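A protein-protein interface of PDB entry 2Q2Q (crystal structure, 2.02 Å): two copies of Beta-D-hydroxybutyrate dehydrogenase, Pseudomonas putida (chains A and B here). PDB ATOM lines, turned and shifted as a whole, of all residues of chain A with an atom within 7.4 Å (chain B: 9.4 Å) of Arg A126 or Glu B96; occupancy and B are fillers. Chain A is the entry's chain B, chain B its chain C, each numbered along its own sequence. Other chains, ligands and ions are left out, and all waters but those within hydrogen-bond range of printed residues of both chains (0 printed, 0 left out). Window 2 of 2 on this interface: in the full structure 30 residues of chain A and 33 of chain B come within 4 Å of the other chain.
Among the printed residues, pairs that only touch across the chains: Phe A115 with Val B95 (3.4 Å), Phe A115 with Phe B98 (3.8 Å), Phe A115 with Trp B103 (3.5 Å), Arg A119 with Val B95 (3.7 Å), Arg A119 with Leu B100 (3.5 Å), Leu A122 with Val B95 (3.6 Å), Leu A122 with Glu B96 (3.7 Å), Pro A123 with Glu B96 (3.97 Å), Val A164 with Lys B148 (3.8 Å), Val A164 with Ala B149 (3.7 Å), Leu A167 with Thr B146 (3.7 Å), Glu A168 with Ala B93 (3.999 Å), Glu A168 with Pro B94 (3.5 Å), Glu A168 with Thr B146 (3.6 Å) and Glu A168 with Lys B148 (3.95 Å).
No position is printed for both chains.
The backbone NH (N) of Val B95 sits at hydrogen-bond distance from the side-chain carboxylate (OE1) of Glu A168, 2.9 Å away.
N of Gly B147 sits at hydrogen-bond distance from OE2 of Glu A168 (2.5 Å).
NE of Arg A126 lies within salt-bridge range of OE1 of Glu B96, 2.8 Å away.
Hydrophobic or aromatic side chains of chain B within 4 Å of the printed part of chain A: Val B95, Phe B98, Leu B100 and Trp B103.
Among the printed residues, 18 pairs touch across the chains.
The backbone NH (N) of Ala B93 is in hydrogen-bond range of the backbone carbonyl oxygen (O) of Gly B147 (3.0 Å).
NH2 of Arg A126 sits at hydrogen-bond distance from O of Glu A168 (3.1 Å).
Arg A126 touches just one residue of chain B: Glu B96 (2.8 Å).
Of chain A, only Leu A122 (3.7 Å), Pro A123 (3.97 Å) and Arg A126 (2.8 Å) come within 4 Å of Glu B96.
Of chain B, only Glu B96 (3.97 Å) comes within 4 Å of Pro A123.
No residue of chain B comes within 4 Å of Ala A127.
Printed residues of chain A within 4 Å of Phe B98: Phe A115.
Of the printed residues of chain B, Phe A115 touches Val B95, Phe B98 and Trp B103.
Of the printed residues of chain A, Ala B93 touches Glu A168.
Printed residues of chain B within 4 Å of Leu A167: Thr B146 (3.7 Å).
Val A165 touches none of the printed residues of chain B.
The nearest residue of chain B that does not touch Arg A126 is Val B95 (5.9 Å).
The nearest residue of chain A that does not touch Glu B96 is Arg A119 (4.02 Å).
The nearest printed residue of chain B that does not touch Val A164 is Gly B147 (4.2 Å).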
ATOM      1  N   PHE A 115     -11.433  27.890 -15.887  1.00  0.00           N
ATOM      2  CA  PHE A 115     -11.252  26.557 -16.526  1.00  0.00           C
ATOM      3  C   PHE A 115     -11.896  26.462 -17.965  1.00  0.00           C
ATOM      4  O   PHE A 115     -11.260  26.047 -18.930  1.00  0.00           O
ATOM      5  CB  PHE A 115     -11.772  25.449 -15.582  1.00  0.00           C
ATOM      6  CG  PHE A 115     -11.958  24.131 -16.258  1.00  0.00           C
ATOM      7  CD1 PHE A 115     -10.866  23.366 -16.669  1.00  0.00           C
ATOM      8  CD2 PHE A 115     -13.254  23.689 -16.544  1.00  0.00           C
ATOM      9  CE1 PHE A 115     -11.062  22.122 -17.353  1.00  0.00           C
ATOM     10  CE2 PHE A 115     -13.502  22.482 -17.214  1.00  0.00           C
ATOM     11  CZ  PHE A 115     -12.395  21.696 -17.619  1.00  0.00           C
ATOM     12  N   THR A 118      -9.971  28.681 -20.468  1.00  0.00           N
ATOM     13  CA  THR A 118      -8.724  28.014 -20.682  1.00  0.00           C
ATOM     14  C   THR A 118      -8.769  26.789 -21.583  1.00  0.00           C
ATOM     15  O   THR A 118      -7.888  26.652 -22.411  1.00  0.00           O
ATOM     16  CB  THR A 118      -7.972  27.704 -19.321  1.00  0.00           C
ATOM     17  OG1 THR A 118      -7.706  28.929 -18.635  1.00  0.00           O
ATOM     18  CG2 THR A 118      -6.684  26.949 -19.531  1.00  0.00           C
ATOM     19  N   ARG A 119      -9.745  25.891 -21.399  1.00  0.00           N
ATOM     20  CA  ARG A 119      -9.737  24.633 -22.118  1.00  0.00           C
ATOM     21  C   ARG A 119     -10.116  24.960 -23.550  1.00  0.00           C
ATOM     22  O   ARG A 119      -9.672  24.325 -24.483  1.00  0.00           O
ATOM     23  CB  ARG A 119     -10.642  23.578 -21.448  1.00  0.00           C
ATOM     24  CG  ARG A 119     -12.155  23.839 -21.649  1.00  0.00           C
ATOM     25  CD  ARG A 119     -13.159  22.905 -20.950  1.00  0.00           C
ATOM     26  NE  ARG A 119     -14.503  23.517 -21.106  1.00  0.00           N
ATOM     27  CZ  ARG A 119     -15.255  23.406 -22.211  1.00  0.00           C
ATOM     28  NH1 ARG A 119     -14.827  22.648 -23.238  1.00  0.00           N
ATOM     29  NH2 ARG A 119     -16.453  24.021 -22.284  1.00  0.00           N
ATOM     30  N   LEU A 120     -10.853  26.055 -23.706  1.00  0.00           N
ATOM     31  CA  LEU A 120     -11.298  26.438 -25.024  1.00  0.00           C
ATOM     32  C   LEU A 120     -10.220  27.127 -25.753  1.00  0.00           C
ATOM     33  O   LEU A 120     -10.213  26.995 -26.945  1.00  0.00           O
ATOM     34  CB  LEU A 120     -12.579  27.294 -25.025  1.00  0.00           C
ATOM     35  CG  LEU A 120     -13.846  26.533 -24.623  1.00  0.00           C
ATOM     36  CD1 LEU A 120     -14.951  27.542 -24.293  1.00  0.00           C
ATOM     37  CD2 LEU A 120     -14.260  25.531 -25.721  1.00  0.00           C
ATOM     38  N   ALA A 121      -9.295  27.844 -25.041  1.00  0.00           N
ATOM     39  CA  ALA A 121      -8.286  28.634 -25.714  1.00  0.00           C
ATOM     40  C   ALA A 121      -7.014  27.877 -26.059  1.00  0.00           C
ATOM     41  O   ALA A 121      -6.359  28.179 -27.033  1.00  0.00           O
ATOM     42  CB  ALA A 121      -7.938  29.907 -24.935  1.00  0.00           C
ATOM     43  N   LEU A 122      -6.658  26.922 -25.236  1.00  0.00           N
ATOM     44  CA  LEU A 122      -5.328  26.356 -25.248  1.00  0.00           C
ATOM     45  C   LEU A 122      -4.931  25.481 -26.458  1.00  0.00           C
ATOM     46  O   LEU A 122      -3.781  25.518 -26.856  1.00  0.00           O
ATOM     47  CB  LEU A 122      -5.081  25.617 -23.916  1.00  0.00           C
ATOM     48  CG  LEU A 122      -3.718  25.010 -23.545  1.00  0.00           C
ATOM     49  CD1 LEU A 122      -2.592  26.059 -23.595  1.00  0.00           C
ATOM     50  CD2 LEU A 122      -3.726  24.374 -22.195  1.00  0.00           C
ATOM     51  N   PRO A 123      -5.835  24.645 -26.985  1.00  0.00           N
ATOM     52  CA  PRO A 123      -5.446  23.867 -28.192  1.00  0.00           C
ATOM     53  C   PRO A 123      -4.952  24.769 -29.316  1.00  0.00           C
ATOM     54  O   PRO A 123      -3.913  24.486 -29.916  1.00  0.00           O
ATOM     55  CB  PRO A 123      -6.721  23.090 -28.535  1.00  0.00           C
ATOM     56  CG  PRO A 123      -7.339  22.893 -27.074  1.00  0.00           C
ATOM     57  CD  PRO A 123      -7.181  24.276 -26.524  1.00  0.00           C
ATOM     58  N   GLY A 124      -5.644  25.887 -29.519  1.00  0.00           N
ATOM     59  CA  GLY A 124      -5.209  26.943 -30.459  1.00  0.00           C
ATOM     60  C   GLY A 124      -3.844  27.597 -30.182  1.00  0.00           C
ATOM     61  O   GLY A 124      -3.035  27.777 -31.089  1.00  0.00           O
ATOM     62  N   MET A 125      -3.609  27.963 -28.938  1.00  0.00           N
ATOM     63  CA  MET A 125      -2.305  28.470 -28.542  1.00  0.00           C
ATOM     64  C   MET A 125      -1.215  27.381 -28.727  1.00  0.00           C
ATOM     65  O   MET A 125      -0.094  27.667 -29.171  1.00  0.00           O
ATOM     66  CB  MET A 125      -2.353  29.020 -27.110  1.00  0.00           C
ATOM     67  CG  MET A 125      -3.397  30.185 -26.865  1.00  0.00           C
ATOM     68  SD  MET A 125      -3.715  30.558 -25.107  1.00  0.00           S
ATOM     69  CE  MET A 125      -4.670  32.057 -25.218  1.00  0.00           C
ATOM     70  N   ARG A 126      -1.502  26.129 -28.394  1.00  0.00           N
ATOM     71  CA  ARG A 126      -0.424  25.196 -28.576  1.00  0.00           C
ATOM     72  C   ARG A 126      -0.158  25.057 -30.107  1.00  0.00           C
ATOM     73  O   ARG A 126       0.988  25.165 -30.558  1.00  0.00           O
ATOM     74  CB  ARG A 126      -0.753  23.825 -27.960  1.00  0.00           C
ATOM     75  CG  ARG A 126      -1.153  23.821 -26.550  1.00  0.00           C
ATOM     76  CD  ARG A 126      -0.995  22.393 -25.907  1.00  0.00           C
ATOM     77  NE  ARG A 126      -1.110  22.317 -24.426  1.00  0.00           N
ATOM     78  CZ  ARG A 126      -0.091  22.165 -23.580  1.00  0.00           C
ATOM     79  NH1 ARG A 126       1.187  22.124 -24.023  1.00  0.00           N
ATOM     80  NH2 ARG A 126      -0.324  22.089 -22.265  1.00  0.00           N
ATOM     81  N   ALA A 127      -1.212  24.855 -30.902  1.00  0.00           N
ATOM     82  CA  ALA A 127      -1.028  24.598 -32.330  1.00  0.00           C
ATOM     83  C   ALA A 127      -0.196  25.721 -32.975  1.00  0.00           C
ATOM     84  O   ALA A 127       0.741  25.458 -33.777  1.00  0.00           O
ATOM     85  CB  ALA A 127      -2.385  24.454 -33.030  1.00  0.00           C
ATOM     86  N   ARG A 128      -0.554  26.963 -32.603  1.00  0.00           N
ATOM     87  CA  ARG A 128       0.108  28.177 -33.102  1.00  0.00           C
ATOM     88  C   ARG A 128       1.510  28.476 -32.464  1.00  0.00           C
ATOM     89  O   ARG A 128       2.123  29.481 -32.836  1.00  0.00           O
ATOM     90  CB  ARG A 128      -0.886  29.379 -33.025  1.00  0.00           C
ATOM     91  CG  ARG A 128      -1.975  29.384 -34.178  1.00  0.00           C
ATOM     92  CD  ARG A 128      -2.937  30.577 -34.113  1.00  0.00           C
ATOM     93  NE  ARG A 128      -3.533  30.710 -32.763  1.00  0.00           N
ATOM     94  CZ  ARG A 128      -4.778  30.340 -32.440  1.00  0.00           C
ATOM     95  NH1 ARG A 128      -5.587  29.788 -33.354  1.00  0.00           N
ATOM     96  NH2 ARG A 128      -5.211  30.491 -31.195  1.00  0.00           N
ATOM     97  N   ASN A 129       2.000  27.572 -31.582  1.00  0.00           N
ATOM     98  CA  ASN A 129       3.114  27.709 -30.568  1.00  0.00           C
ATOM     99  C   ASN A 129       3.359  29.116 -30.031  1.00  0.00           C
ATOM    100  O   ASN A 129       4.476  29.568 -30.050  1.00  0.00           O
ATOM    101  CB  ASN A 129       4.486  27.034 -30.985  1.00  0.00           C
ATOM    102  CG  ASN A 129       5.336  26.473 -29.772  1.00  0.00           C
ATOM    103  OD1 ASN A 129       4.957  26.423 -28.506  1.00  0.00           O
ATOM    104  ND2 ASN A 129       6.542  26.057 -30.156  1.00  0.00           N
ATOM    105  N   TRP A 130       2.280  29.772 -29.583  1.00  0.00           N
ATOM    106  CA  TRP A 130       2.383  30.996 -28.837  1.00  0.00           C
ATOM    107  C   TRP A 130       1.039  31.217 -28.193  1.00  0.00           C
ATOM    108  O   TRP A 130       0.033  30.947 -28.811  1.00  0.00           O
ATOM    109  CB  TRP A 130       2.752  32.150 -29.766  1.00  0.00           C
ATOM    110  CG  TRP A 130       3.225  33.384 -28.919  1.00  0.00           C
ATOM    111  CD1 TRP A 130       4.461  33.672 -28.565  1.00  0.00           C
ATOM    112  CD2 TRP A 130       2.369  34.427 -28.354  1.00  0.00           C
ATOM    113  NE1 TRP A 130       4.498  34.867 -27.848  1.00  0.00           N
ATOM    114  CE2 TRP A 130       3.207  35.339 -27.704  1.00  0.00           C
ATOM    115  CE3 TRP A 130       0.982  34.674 -28.394  1.00  0.00           C
ATOM    116  CZ2 TRP A 130       2.738  36.481 -27.080  1.00  0.00           C
ATOM    117  CZ3 TRP A 130       0.471  35.839 -27.722  1.00  0.00           C
ATOM    118  CH2 TRP A 130       1.362  36.723 -27.081  1.00  0.00           C
ATOM    119  N   GLY A 131       1.010  31.588 -26.907  1.00  0.00           N
ATOM    120  CA  GLY A 131      -0.207  31.957 -26.220  1.00  0.00           C
ATOM    121  C   GLY A 131       0.028  32.653 -24.888  1.00  0.00           C
ATOM    122  O   GLY A 131       1.062  32.512 -24.261  1.00  0.00           O
ATOM    123  N   VAL A 164      -1.404  25.008 -12.250  1.00  0.00           N
ATOM    124  CA  VAL A 164      -1.463  23.741 -13.060  1.00  0.00           C
ATOM    125  C   VAL A 164      -1.249  24.004 -14.544  1.00  0.00           C
ATOM    126  O   VAL A 164      -0.473  23.304 -15.199  1.00  0.00           O
ATOM    127  CB  VAL A 164      -2.773  22.932 -12.828  1.00  0.00           C
ATOM    128  CG1 VAL A 164      -2.872  21.718 -13.754  1.00  0.00           C
ATOM    129  CG2 VAL A 164      -2.810  22.483 -11.370  1.00  0.00           C
ATOM    130  N   VAL A 165      -1.901  25.048 -15.058  1.00  0.00           N
ATOM    131  CA  VAL A 165      -1.844  25.330 -16.494  1.00  0.00           C
ATOM    132  C   VAL A 165      -0.454  25.831 -16.802  1.00  0.00           C
ATOM    133  O   VAL A 165       0.223  25.301 -17.683  1.00  0.00           O
ATOM    134  CB  VAL A 165      -2.929  26.355 -16.938  1.00  0.00           C
ATOM    135  CG1 VAL A 165      -2.851  26.585 -18.459  1.00  0.00           C
ATOM    136  CG2 VAL A 165      -4.277  25.806 -16.583  1.00  0.00           C
ATOM    137  N   LEU A 167       2.226  24.956 -15.292  1.00  0.00           N
ATOM    138  CA  LEU A 167       3.176  23.807 -15.389  1.00  0.00           C
ATOM    139  C   LEU A 167       2.923  23.030 -16.627  1.00  0.00           C
ATOM    140  O   LEU A 167       3.837  22.510 -17.258  1.00  0.00           O
ATOM    141  CB  LEU A 167       2.998  22.818 -14.202  1.00  0.00           C
ATOM    142  CG  LEU A 167       3.387  23.519 -12.934  1.00  0.00           C
ATOM    143  CD1 LEU A 167       2.838  22.824 -11.655  1.00  0.00           C
ATOM    144  CD2 LEU A 167       4.964  23.691 -12.875  1.00  0.00           C
ATOM    145  N   GLU A 168       1.633  22.852 -16.972  1.00  0.00           N
ATOM    146  CA  GLU A 168       1.326  21.998 -18.128  1.00  0.00           C
ATOM    147  C   GLU A 168       1.854  22.537 -19.466  1.00  0.00           C
ATOM    148  O   GLU A 168       2.105  21.750 -20.420  1.00  0.00           O
ATOM    149  CB  GLU A 168      -0.182  21.632 -18.196  1.00  0.00           C
ATOM    150  CG  GLU A 168      -0.603  20.568 -17.170  1.00  0.00           C
ATOM    151  CD  GLU A 168      -2.126  20.298 -17.146  1.00  0.00           C
ATOM    152  OE1 GLU A 168      -2.826  20.789 -18.074  1.00  0.00           O
ATOM    153  OE2 GLU A 168      -2.636  19.612 -16.188  1.00  0.00           O
ATOM    154  N   THR A 169       1.971  23.878 -19.539  1.00  0.00           N
ATOM    155  CA  THR A 169       2.413  24.568 -20.748  1.00  0.00           C
ATOM    156  C   THR A 169       3.850  25.018 -20.679  1.00  0.00           C
ATOM    157  O   THR A 169       4.313  25.753 -21.590  1.00  0.00           O
ATOM    158  CB  THR A 169       1.531  25.862 -21.028  1.00  0.00           C
ATOM    159  OG1 THR A 169       1.564  26.673 -19.871  1.00  0.00           O
ATOM    160  CG2 THR A 169       0.102  25.599 -21.287  1.00  0.00           C
ATOM    161  N   ALA A 170       4.591  24.546 -19.672  1.00  0.00           N
ATOM    162  CA  ALA A 170       5.911  25.130 -19.342  1.00  0.00           C
ATOM    163  C   ALA A 170       6.966  24.860 -20.365  1.00  0.00           C
ATOM    164  O   ALA A 170       7.799  25.715 -20.580  1.00  0.00           O
ATOM    165  CB  ALA A 170       6.424  24.753 -17.930  1.00  0.00           C
ATOM    166  N   THR A 171       6.862  23.714 -21.073  1.00  0.00           N
ATOM    167  CA  THR A 171       7.789  23.441 -22.122  1.00  0.00           C
ATOM    168  C   THR A 171       7.305  24.078 -23.456  1.00  0.00           C
ATOM    169  O   THR A 171       7.713  23.650 -24.510  1.00  0.00           O
ATOM    170  CB  THR A 171       8.071  21.933 -22.289  1.00  0.00           C
ATOM    171  OG1 THR A 171       6.841  21.232 -22.538  1.00  0.00           O
ATOM    172  CG2 THR A 171       8.694  21.340 -21.013  1.00  0.00           C
ATOM    173  N   SER A 172       6.458  25.104 -23.433  1.00  0.00           N
ATOM    174  CA  SER A 172       5.936  25.578 -24.725  1.00  0.00           C
ATOM    175  C   SER A 172       6.144  27.059 -24.663  1.00  0.00           C
ATOM    176  O   SER A 172       6.562  27.573 -23.585  1.00  0.00           O
ATOM    177  CB  SER A 172       4.449  25.196 -24.858  1.00  0.00           C
ATOM    178  OG  SER A 172       3.619  25.889 -23.894  1.00  0.00           O
ATOM    179  N   ASN A 173       5.865  27.764 -25.769  1.00  0.00           N
ATOM    180  CA  ASN A 173       5.792  29.235 -25.769  1.00  0.00           C
ATOM    181  C   ASN A 173       4.394  29.735 -25.363  1.00  0.00           C
ATOM    182  O   ASN A 173       4.114  30.908 -25.491  1.00  0.00           O
ATOM    183  CB  ASN A 173       6.312  29.903 -27.081  1.00  0.00           C
ATOM    184  CG  ASN A 173       7.514  29.197 -27.679  1.00  0.00           C
ATOM    185  OD1 ASN A 173       8.377  28.700 -26.953  1.00  0.00           O
ATOM    186  ND2 ASN A 173       7.532  29.056 -29.034  1.00  0.00           N
ATOM    187  N   VAL A 174       3.575  28.886 -24.753  1.00  0.00           N
ATOM    188  CA  VAL A 174       2.330  29.312 -23.973  1.00  0.00           C
ATOM    189  C   VAL A 174       2.580  29.438 -22.454  1.00  0.00           C
ATOM    190  O   VAL A 174       3.067  28.523 -21.792  1.00  0.00           O
ATOM    191  CB  VAL A 174       1.072  28.439 -24.271  1.00  0.00           C
ATOM    192  CG1 VAL A 174      -0.201  28.933 -23.587  1.00  0.00           C
ATOM    193  CG2 VAL A 174       0.834  28.270 -25.777  1.00  0.00           C
ATOM    194  N   ALA B  93      -5.950  14.448 -15.715  1.00  0.00           N
ATOM    195  CA  ALA B  93      -5.912  14.735 -17.144  1.00  0.00           C
ATOM    196  C   ALA B  93      -5.415  16.177 -17.371  1.00  0.00           C
ATOM    197  O   ALA B  93      -5.703  17.075 -16.576  1.00  0.00           O
ATOM    198  CB  ALA B  93      -7.319  14.527 -17.801  1.00  0.00           C
ATOM    199  N   PRO B  94      -4.686  16.401 -18.472  1.00  0.00           N
ATOM    200  CA  PRO B  94      -4.369  17.742 -18.930  1.00  0.00           C
ATOM    201  C   PRO B  94      -5.609  18.619 -19.062  1.00  0.00           C
ATOM    202  O   PRO B  94      -6.648  18.149 -19.546  1.00  0.00           O
ATOM    203  CB  PRO B  94      -3.780  17.487 -20.338  1.00  0.00           C
ATOM    204  CG  PRO B  94      -4.107  16.052 -20.637  1.00  0.00           C
ATOM    205  CD  PRO B  94      -4.086  15.380 -19.355  1.00  0.00           C
ATOM    206  N   VAL B  95      -5.479  19.888 -18.743  1.00  0.00           N
ATOM    207  CA  VAL B  95      -6.615  20.793 -18.593  1.00  0.00           C
ATOM    208  C   VAL B  95      -7.562  20.815 -19.796  1.00  0.00           C
ATOM    209  O   VAL B  95      -8.809  20.900 -19.636  1.00  0.00           O
ATOM    210  CB  VAL B  95      -6.186  22.253 -18.184  1.00  0.00           C
ATOM    211  CG1 VAL B  95      -5.357  22.948 -19.273  1.00  0.00           C
ATOM    212  CG2 VAL B  95      -7.423  23.101 -17.865  1.00  0.00           C
ATOM    213  N   GLU B  96      -6.992  20.758 -20.997  1.00  0.00           N
ATOM    214  CA  GLU B  96      -7.808  20.825 -22.200  1.00  0.00           C
ATOM    215  C   GLU B  96      -8.482  19.495 -22.557  1.00  0.00           C
ATOM    216  O   GLU B  96      -9.289  19.451 -23.507  1.00  0.00           O
ATOM    217  CB  GLU B  96      -7.015  21.390 -23.413  1.00  0.00           C
ATOM    218  CG  GLU B  96      -5.885  20.492 -23.957  1.00  0.00           C
ATOM    219  CD  GLU B  96      -4.536  20.747 -23.266  1.00  0.00           C
ATOM    220  OE1 GLU B  96      -3.545  20.990 -23.993  1.00  0.00           O
ATOM    221  OE2 GLU B  96      -4.462  20.706 -22.012  1.00  0.00           O
ATOM    222  N   GLN B  97      -8.133  18.434 -21.818  1.00  0.00           N
ATOM    223  CA  GLN B  97      -8.737  17.101 -21.999  1.00  0.00           C
ATOM    224  C   GLN B  97      -9.439  16.729 -20.676  1.00  0.00           C
ATOM    225  O   GLN B  97      -9.630  15.561 -20.373  1.00  0.00           O
ATOM    226  CB  GLN B  97      -7.684  16.022 -22.365  1.00  0.00           C
ATOM    227  CG  GLN B  97      -7.217  15.921 -23.829  1.00  0.00           C
ATOM    228  CD  GLN B  97      -8.377  15.676 -24.796  1.00  0.00           C
ATOM    229  OE1 GLN B  97      -9.220  16.569 -24.999  1.00  0.00           O
ATOM    230  NE2 GLN B  97      -8.440  14.461 -25.398  1.00  0.00           N
ATOM    231  N   PHE B  98      -9.798  17.721 -19.867  1.00  0.00           N
ATOM    232  CA  PHE B  98     -10.310  17.436 -18.530  1.00  0.00           C
ATOM    233  C   PHE B  98     -11.826  17.354 -18.699  1.00  0.00           C
ATOM    234  O   PHE B  98     -12.405  18.219 -19.385  1.00  0.00           O
ATOM    235  CB  PHE B  98      -9.882  18.508 -17.499  1.00  0.00           C
ATOM    236  CG  PHE B  98      -9.856  18.016 -16.098  1.00  0.00           C
ATOM    237  CD1 PHE B  98      -8.647  17.746 -15.459  1.00  0.00           C
ATOM    238  CD2 PHE B  98     -11.040  17.817 -15.388  1.00  0.00           C
ATOM    239  CE1 PHE B  98      -8.598  17.305 -14.121  1.00  0.00           C
ATOM    240  CE2 PHE B  98     -11.011  17.382 -14.047  1.00  0.00           C
ATOM    241  CZ  PHE B  98      -9.784  17.106 -13.417  1.00  0.00           C
ATOM    242  N   PRO B  99     -12.453  16.256 -18.208  1.00  0.00           N
ATOM    243  CA  PRO B  99     -13.856  16.034 -18.485  1.00  0.00           C
ATOM    244  C   PRO B  99     -14.734  17.017 -17.734  1.00  0.00           C
ATOM    245  O   PRO B  99     -14.457  17.383 -16.607  1.00  0.00           O
ATOM    246  CB  PRO B  99     -14.065  14.577 -18.034  1.00  0.00           C
ATOM    247  CG  PRO B  99     -12.689  13.976 -18.064  1.00  0.00           C
ATOM    248  CD  PRO B  99     -11.890  15.116 -17.469  1.00  0.00           C
ATOM    249  N   LEU B 100     -15.722  17.546 -18.409  1.00  0.00           N
ATOM    250  CA  LEU B 100     -16.423  18.675 -17.869  1.00  0.00           C
ATOM    251  C   LEU B 100     -17.153  18.299 -16.588  1.00  0.00           C
ATOM    252  O   LEU B 100     -17.176  19.071 -15.649  1.00  0.00           O
ATOM    253  CB  LEU B 100     -17.357  19.225 -18.938  1.00  0.00           C
ATOM    254  CG  LEU B 100     -16.793  20.376 -19.791  1.00  0.00           C
ATOM    255  CD1 LEU B 100     -15.260  20.258 -20.185  1.00  0.00           C
ATOM    256  CD2 LEU B 100     -17.759  20.781 -20.952  1.00  0.00           C
ATOM    257  N   TRP B 103     -14.677  17.992 -13.699  1.00  0.00           N
ATOM    258  CA  TRP B 103     -14.406  19.299 -13.152  1.00  0.00           C
ATOM    259  C   TRP B 103     -15.535  19.709 -12.152  1.00  0.00           C
ATOM    260  O   TRP B 103     -15.260  19.991 -11.002  1.00  0.00           O
ATOM    261  CB  TRP B 103     -14.333  20.303 -14.285  1.00  0.00           C
ATOM    262  CG  TRP B 103     -14.301  21.719 -13.696  1.00  0.00           C
ATOM    263  CD1 TRP B 103     -15.382  22.541 -13.432  1.00  0.00           C
ATOM    264  CD2 TRP B 103     -13.132  22.428 -13.254  1.00  0.00           C
ATOM    265  NE1 TRP B 103     -14.921  23.724 -12.823  1.00  0.00           N
ATOM    266  CE2 TRP B 103     -13.558  23.691 -12.748  1.00  0.00           C
ATOM    267  CE3 TRP B 103     -11.750  22.139 -13.277  1.00  0.00           C
ATOM    268  CZ2 TRP B 103     -12.631  24.670 -12.226  1.00  0.00           C
ATOM    269  CZ3 TRP B 103     -10.843  23.091 -12.763  1.00  0.00           C
ATOM    270  CH2 TRP B 103     -11.293  24.362 -12.273  1.00  0.00           C
ATOM    271  N   THR B 146       0.952  18.894 -12.633  1.00  0.00           N
ATOM    272  CA  THR B 146       0.343  18.638 -13.926  1.00  0.00           C
ATOM    273  C   THR B 146      -0.779  17.633 -13.781  1.00  0.00           C
ATOM    274  O   THR B 146      -0.725  16.785 -12.878  1.00  0.00           O
ATOM    275  CB  THR B 146       1.430  18.124 -14.900  1.00  0.00           C
ATOM    276  OG1 THR B 146       2.056  17.010 -14.283  1.00  0.00           O
ATOM    277  CG2 THR B 146       2.542  19.233 -14.932  1.00  0.00           C
ATOM    278  N   GLY B 147      -1.795  17.770 -14.643  1.00  0.00           N
ATOM    279  CA  GLY B 147      -2.942  16.881 -14.666  1.00  0.00           C
ATOM    280  C   GLY B 147      -4.038  17.120 -13.649  1.00  0.00           C
ATOM    281  O   GLY B 147      -5.033  16.355 -13.655  1.00  0.00           O
ATOM    282  N   LYS B 148      -3.876  18.111 -12.748  1.00  0.00           N
ATOM    283  CA  LYS B 148      -4.751  18.218 -11.588  1.00  0.00           C
ATOM    284  C   LYS B 148      -5.489  19.517 -11.524  1.00  0.00           C
ATOM    285  O   LYS B 148      -5.663  20.071 -10.467  1.00  0.00           O
ATOM    286  CB  LYS B 148      -3.999  17.938 -10.277  1.00  0.00           C
ATOM    287  CG  LYS B 148      -3.359  16.571 -10.277  1.00  0.00           C
ATOM    288  CD  LYS B 148      -2.793  16.142  -8.926  1.00  0.00           C
ATOM    289  CE  LYS B 148      -2.589  14.590  -9.023  1.00  0.00           C
ATOM    290  NZ  LYS B 148      -1.400  14.022  -8.276  1.00  0.00           N
ATOM    291  N   ALA B 149      -5.980  19.973 -12.660  1.00  0.00           N
ATOM    292  CA  ALA B 149      -6.612  21.273 -12.773  1.00  0.00           C
ATOM    293  C   ALA B 149      -7.669  21.388 -11.663  1.00  0.00           C
ATOM    294  O   ALA B 149      -7.564  22.216 -10.822  1.00  0.00           O
ATOM    295  CB  ALA B 149      -7.271  21.372 -14.164  1.00  0.00           C
